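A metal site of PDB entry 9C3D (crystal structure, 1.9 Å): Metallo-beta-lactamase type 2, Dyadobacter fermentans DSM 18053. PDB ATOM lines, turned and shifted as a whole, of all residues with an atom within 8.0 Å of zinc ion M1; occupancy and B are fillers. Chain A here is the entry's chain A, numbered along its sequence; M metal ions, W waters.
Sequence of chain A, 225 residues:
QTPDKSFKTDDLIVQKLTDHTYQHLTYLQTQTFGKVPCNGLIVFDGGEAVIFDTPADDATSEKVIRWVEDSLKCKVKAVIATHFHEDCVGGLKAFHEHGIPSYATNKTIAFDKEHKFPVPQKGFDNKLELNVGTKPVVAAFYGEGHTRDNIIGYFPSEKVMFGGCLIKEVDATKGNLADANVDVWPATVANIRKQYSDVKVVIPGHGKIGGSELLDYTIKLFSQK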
ATOM      1  N   ASP A  53     -22.903   3.739 -12.650  1.00  0.00           N
ATOM      2  CA  ASP A  53     -22.699   2.315 -12.363  1.00  0.00           C
ATOM      3  C   ASP A  53     -21.759   2.117 -11.179  1.00  0.00           C
ATOM      4  O   ASP A  53     -20.718   2.762 -11.087  1.00  0.00           O
ATOM      5  CB  ASP A  53     -22.137   1.564 -13.585  1.00  0.00           C
ATOM      6  CG  ASP A  53     -23.198   1.237 -14.615  1.00  0.00           C
ATOM      7  OD1 ASP A  53     -24.365   1.679 -14.496  1.00  0.00           O
ATOM      8  OD2 ASP A  53     -22.850   0.522 -15.584  1.00  0.00           O
ATOM      9  N   THR A  82     -27.356   2.351 -14.371  1.00  0.00           N
ATOM     10  CA  THR A  82     -27.873   2.563 -15.726  1.00  0.00           C
ATOM     11  C   THR A  82     -28.700   1.402 -16.261  1.00  0.00           C
ATOM     12  O   THR A  82     -29.378   1.579 -17.282  1.00  0.00           O
ATOM     13  CB  THR A  82     -26.740   2.893 -16.704  1.00  0.00           C
ATOM     14  OG1 THR A  82     -25.789   1.829 -16.742  1.00  0.00           O
ATOM     15  CG2 THR A  82     -26.022   4.177 -16.275  1.00  0.00           C
ATOM     16  N   HIS A  83     -28.674   0.234 -15.618  1.00  0.00           N
ATOM     17  CA  HIS A  83     -29.741  -0.755 -15.736  1.00  0.00           C
ATOM     18  C   HIS A  83     -29.611  -1.725 -14.561  1.00  0.00           C
ATOM     19  O   HIS A  83     -28.779  -1.535 -13.677  1.00  0.00           O
ATOM     20  CB  HIS A  83     -29.730  -1.475 -17.104  1.00  0.00           C
ATOM     21  CG  HIS A  83     -28.546  -2.345 -17.344  1.00  0.00           C
ATOM     22  ND1 HIS A  83     -27.362  -1.864 -17.847  1.00  0.00           N
ATOM     23  CD2 HIS A  83     -28.372  -3.682 -17.202  1.00  0.00           C
ATOM     24  CE1 HIS A  83     -26.503  -2.861 -17.998  1.00  0.00           C
ATOM     25  NE2 HIS A  83     -27.089  -3.971 -17.597  1.00  0.00           N
ATOM     26  N   PHE A  84     -30.467  -2.755 -14.540  1.00  0.00           N
ATOM     27  CA  PHE A  84     -30.624  -3.508 -13.308  1.00  0.00           C
ATOM     28  C   PHE A  84     -29.570  -4.585 -13.100  1.00  0.00           C
ATOM     29  O   PHE A  84     -29.501  -5.135 -11.993  1.00  0.00           O
ATOM     30  CB  PHE A  84     -32.034  -4.133 -13.246  1.00  0.00           C
ATOM     31  CG  PHE A  84     -32.226  -5.350 -14.128  1.00  0.00           C
ATOM     32  CD1 PHE A  84     -32.597  -5.209 -15.454  1.00  0.00           C
ATOM     33  CD2 PHE A  84     -32.089  -6.640 -13.611  1.00  0.00           C
ATOM     34  CE1 PHE A  84     -32.799  -6.327 -16.265  1.00  0.00           C
ATOM     35  CE2 PHE A  84     -32.291  -7.764 -14.410  1.00  0.00           C
ATOM     36  CZ  PHE A  84     -32.646  -7.607 -15.736  1.00  0.00           C
ATOM     37  N   HIS A  85     -28.743  -4.894 -14.092  1.00  0.00           N
ATOM     38  CA  HIS A  85     -27.796  -5.997 -13.966  1.00  0.00           C
ATOM     39  C   HIS A  85     -26.704  -5.688 -12.931  1.00  0.00           C
ATOM     40  O   HIS A  85     -26.489  -4.544 -12.533  1.00  0.00           O
ATOM     41  CB  HIS A  85     -27.185  -6.321 -15.320  1.00  0.00           C
ATOM     42  CG  HIS A  85     -28.103  -7.080 -16.229  1.00  0.00           C
ATOM     43  ND1 HIS A  85     -27.915  -7.144 -17.593  1.00  0.00           N
ATOM     44  CD2 HIS A  85     -29.203  -7.821 -15.968  1.00  0.00           C
ATOM     45  CE1 HIS A  85     -28.863  -7.869 -18.144  1.00  0.00           C
ATOM     46  NE2 HIS A  85     -29.656  -8.303 -17.172  1.00  0.00           N
ATOM     47  N   GLU A  86     -26.007  -6.750 -12.515  1.00  0.00           N
ATOM     48  CA  GLU A  86     -25.031  -6.642 -11.432  1.00  0.00           C
ATOM     49  C   GLU A  86     -23.779  -5.840 -11.802  1.00  0.00           C
ATOM     50  O   GLU A  86     -23.077  -5.378 -10.902  1.00  0.00           O
ATOM     51  CB  GLU A  86     -24.629  -8.036 -10.943  1.00  0.00           C
ATOM     52  CG  GLU A  86     -25.750  -8.783 -10.217  1.00  0.00           C
ATOM     53  CD  GLU A  86     -25.260 -10.021  -9.510  1.00  0.00           C
ATOM     54  OE1 GLU A  86     -24.051 -10.346  -9.631  1.00  0.00           O
ATOM     55  OE2 GLU A  86     -26.076 -10.677  -8.819  1.00  0.00           O
ATOM     56  N   ASP A  87     -23.478  -5.636 -13.098  1.00  0.00           N
ATOM     57  CA  ASP A  87     -22.377  -4.718 -13.399  1.00  0.00           C
ATOM     58  C   ASP A  87     -22.792  -3.248 -13.290  1.00  0.00           C
ATOM     59  O   ASP A  87     -22.018  -2.355 -13.680  1.00  0.00           O
ATOM     60  CB  ASP A  87     -21.755  -5.020 -14.774  1.00  0.00           C
ATOM     61  CG  ASP A  87     -22.762  -5.110 -15.911  1.00  0.00           C
ATOM     62  OD1 ASP A  87     -23.873  -5.655 -15.695  1.00  0.00           O
ATOM     63  OD2 ASP A  87     -22.427  -4.666 -17.044  1.00  0.00           O
ATOM     64  N   CYS A  88     -23.998  -2.984 -12.751  1.00  0.00           N
ATOM     65  CA  CYS A  88     -24.474  -1.630 -12.492  1.00  0.00           C
ATOM     66  C   CYS A  88     -24.823  -1.393 -11.019  1.00  0.00           C
ATOM     67  O   CYS A  88     -24.689  -0.255 -10.565  1.00  0.00           O
ATOM     68  CB  CYS A  88     -25.713  -1.302 -13.335  1.00  0.00           C
ATOM     69  SG  CYS A  88     -25.545  -1.746 -15.067  1.00  0.00           S
ATOM     70  N   HIS A 146     -30.167  -3.400 -24.801  1.00  0.00           N
ATOM     71  CA  HIS A 146     -29.512  -4.422 -24.007  1.00  0.00           C
ATOM     72  C   HIS A 146     -30.469  -4.975 -22.948  1.00  0.00           C
ATOM     73  O   HIS A 146     -30.477  -6.177 -22.668  1.00  0.00           O
ATOM     74  CB  HIS A 146     -28.275  -3.824 -23.352  1.00  0.00           C
ATOM     75  CG  HIS A 146     -27.587  -4.776 -22.440  1.00  0.00           C
ATOM     76  ND1 HIS A 146     -26.852  -5.842 -22.914  1.00  0.00           N
ATOM     77  CD2 HIS A 146     -27.503  -4.830 -21.095  1.00  0.00           C
ATOM     78  CE1 HIS A 146     -26.353  -6.525 -21.897  1.00  0.00           C
ATOM     79  NE2 HIS A 146     -26.743  -5.938 -20.779  1.00  0.00           N
ATOM     80  N   THR A 147     -31.263  -4.104 -22.344  1.00  0.00           N
ATOM     81  CA  THR A 147     -32.348  -4.496 -21.466  1.00  0.00           C
ATOM     82  C   THR A 147     -33.521  -3.566 -21.750  1.00  0.00           C
ATOM     83  O   THR A 147     -33.395  -2.591 -22.481  1.00  0.00           O
ATOM     84  CB  THR A 147     -31.951  -4.375 -19.998  1.00  0.00           C
ATOM     85  OG1 THR A 147     -31.551  -3.018 -19.734  1.00  0.00           O
ATOM     86  CG2 THR A 147     -30.816  -5.335 -19.649  1.00  0.00           C
ATOM     87  N   ASP A 149     -34.807  -1.611 -19.624  1.00  0.00           N
ATOM     88  CA  ASP A 149     -34.697  -0.451 -18.754  1.00  0.00           C
ATOM     89  C   ASP A 149     -33.459   0.425 -18.987  1.00  0.00           C
ATOM     90  O   ASP A 149     -33.311   1.448 -18.314  1.00  0.00           O
ATOM     91  CB  ASP A 149     -34.721  -0.909 -17.286  1.00  0.00           C
ATOM     92  CG  ASP A 149     -33.529  -1.800 -16.934  1.00  0.00           C
ATOM     93  OD1 ASP A 149     -33.141  -2.643 -17.772  1.00  0.00           O
ATOM     94  OD2 ASP A 149     -32.952  -1.642 -15.824  1.00  0.00           O
ATOM     95  N   ASN A 150     -32.552   0.054 -19.895  1.00  0.00           N
ATOM     96  CA  ASN A 150     -31.229   0.680 -19.898  1.00  0.00           C
ATOM     97  C   ASN A 150     -31.294   2.171 -20.250  1.00  0.00           C
ATOM     98  O   ASN A 150     -32.048   2.586 -21.130  1.00  0.00           O
ATOM     99  CB  ASN A 150     -30.250  -0.034 -20.850  1.00  0.00           C
ATOM    100  CG  ASN A 150     -30.833  -0.347 -22.222  1.00  0.00           C
ATOM    101  OD1 ASN A 150     -30.381  -1.287 -22.890  1.00  0.00           O
ATOM    102  ND2 ASN A 150     -31.818   0.440 -22.672  1.00  0.00           N
ATOM    103  N   GLY A 164     -23.096   2.667 -21.294  1.00  0.00           N
ATOM    104  CA  GLY A 164     -23.494   1.445 -20.647  1.00  0.00           C
ATOM    105  C   GLY A 164     -23.587   0.292 -21.627  1.00  0.00           C
ATOM    106  O   GLY A 164     -23.076   0.341 -22.749  1.00  0.00           O
ATOM    107  N   CYS A 165     -24.283  -0.757 -21.204  1.00  0.00           N
ATOM    108  CA  CYS A 165     -24.251  -1.953 -22.035  1.00  0.00           C
ATOM    109  C   CYS A 165     -25.131  -1.835 -23.265  1.00  0.00           C
ATOM    110  O   CYS A 165     -25.070  -2.723 -24.130  1.00  0.00           O
ATOM    111  CB  CYS A 165     -24.607  -3.151 -21.175  1.00  0.00           C
ATOM    112  SG  CYS A 165     -23.509  -3.208 -19.711  1.00  0.00           S
ATOM    113  N   LEU A 166     -25.897  -0.743 -23.380  1.00  0.00           N
ATOM    114  CA  LEU A 166     -26.632  -0.442 -24.604  1.00  0.00           C
ATOM    115  C   LEU A 166     -25.689  -0.176 -25.763  1.00  0.00           C
ATOM    116  O   LEU A 166     -26.062  -0.344 -26.927  1.00  0.00           O
ATOM    117  CB  LEU A 166     -27.529   0.774 -24.372  1.00  0.00           C
ATOM    118  CG  LEU A 166     -28.441   1.289 -25.505  1.00  0.00           C
ATOM    119  CD1 LEU A 166     -29.462   0.211 -25.939  1.00  0.00           C
ATOM    120  CD2 LEU A 166     -29.154   2.561 -25.089  1.00  0.00           C
ATOM    121  N   LYS A 168     -21.985  -0.843 -27.558  1.00  0.00           N
ATOM    122  CA  LYS A 168     -20.904  -1.805 -27.683  1.00  0.00           C
ATOM    123  C   LYS A 168     -19.628  -1.130 -28.156  1.00  0.00           C
ATOM    124  O   LYS A 168     -19.680  -0.166 -28.934  1.00  0.00           O
ATOM    125  CB  LYS A 168     -21.284  -2.914 -28.675  1.00  0.00           C
ATOM    126  CG  LYS A 168     -22.523  -3.679 -28.269  1.00  0.00           C
ATOM    127  CD  LYS A 168     -22.243  -4.461 -26.982  1.00  0.00           C
ATOM    128  CE  LYS A 168     -23.415  -5.364 -26.621  1.00  0.00           C
ATOM    129  NZ  LYS A 168     -23.069  -6.170 -25.414  1.00  0.00           N
ATOM    130  N   ASN A 176     -24.427 -10.621 -24.192  1.00  0.00           N
ATOM    131  CA  ASN A 176     -25.497 -11.292 -23.459  1.00  0.00           C
ATOM    132  C   ASN A 176     -26.831 -10.685 -23.872  1.00  0.00           C
ATOM    133  O   ASN A 176     -27.092  -9.516 -23.587  1.00  0.00           O
ATOM    134  CB  ASN A 176     -25.282 -11.144 -21.953  1.00  0.00           C
ATOM    135  CG  ASN A 176     -26.531 -11.460 -21.140  1.00  0.00           C
ATOM    136  OD1 ASN A 176     -27.261 -12.380 -21.459  1.00  0.00           O
ATOM    137  ND2 ASN A 176     -26.770 -10.677 -20.082  1.00  0.00           N
ATOM    138  N   ASP A 179     -31.846 -10.549 -21.677  1.00  0.00           N
ATOM    139  CA  ASP A 179     -32.883  -9.592 -21.314  1.00  0.00           C
ATOM    140  C   ASP A 179     -33.123  -8.567 -22.406  1.00  0.00           C
ATOM    141  O   ASP A 179     -33.799  -7.551 -22.163  1.00  0.00           O
ATOM    142  CB  ASP A 179     -32.508  -8.887 -20.002  1.00  0.00           C
ATOM    143  CG  ASP A 179     -32.431  -9.847 -18.829  1.00  0.00           C
ATOM    144  OD1 ASP A 179     -33.355 -10.660 -18.670  1.00  0.00           O
ATOM    145  OD2 ASP A 179     -31.430  -9.844 -18.094  1.00  0.00           O
ATOM    146  N   GLY A 205     -20.438  -0.155 -22.135  1.00  0.00           N
ATOM    147  CA  GLY A 205     -20.542  -0.917 -20.903  1.00  0.00           C
ATOM    148  C   GLY A 205     -19.343  -1.817 -20.676  1.00  0.00           C
ATOM    149  O   GLY A 205     -18.929  -2.022 -19.531  1.00  0.00           O
ATOM    150  N   HIS A 206     -18.774  -2.337 -21.765  1.00  0.00           N
ATOM    151  CA  HIS A 206     -17.574  -3.156 -21.728  1.00  0.00           C
ATOM    152  C   HIS A 206     -16.673  -2.802 -22.901  1.00  0.00           C
ATOM    153  O   HIS A 206     -17.146  -2.638 -24.025  1.00  0.00           O
ATOM    154  CB  HIS A 206     -17.905  -4.651 -21.797  1.00  0.00           C
ATOM    155  CG  HIS A 206     -19.000  -5.071 -20.861  1.00  0.00           C
ATOM    156  ND1 HIS A 206     -18.758  -5.509 -19.578  1.00  0.00           N
ATOM    157  CD2 HIS A 206     -20.344  -5.128 -21.039  1.00  0.00           C
ATOM    158  CE1 HIS A 206     -19.906  -5.815 -19.006  1.00  0.00           C
ATOM    159  NE2 HIS A 206     -20.887  -5.591 -19.859  1.00  0.00           N
HETATM  160 ZN    ZN M   1     -26.340  -5.886 -18.591  1.00  0.00          ZN
HETATM  161 ZN    ZN M   2     -23.061  -5.356 -19.176  1.00  0.00          ZN
HETATM  162  O   HOH W   1     -24.588  -6.266 -18.071  1.00  0.00           O
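Zinc ion M1 is bound by water W1 (1.9 Å), a ring nitrogen (NE2) of His 146 (2.2 Å), a ring nitrogen (ND1) of His 85 (2.2 Å) and a ring nitrogen (NE2) of His 83 (2.3 Å).
Residues that only touch zinc ion M1: Asp 87 (3.8 Å).
Four residues have an atom within 4 Å of zinc ion M1: His 83, His 85, Asp 87 and His 146.
N of His 146 is in hydrogen-bond range of OD1 of Asn 150, at 2.9 Å.
NE2 of His 85 is in hydrogen-bond range of OD2 of Asp 179 (2.5 Å).
ND1 of His 83 lies close to SG of Cys 88, at 3.3 Å.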
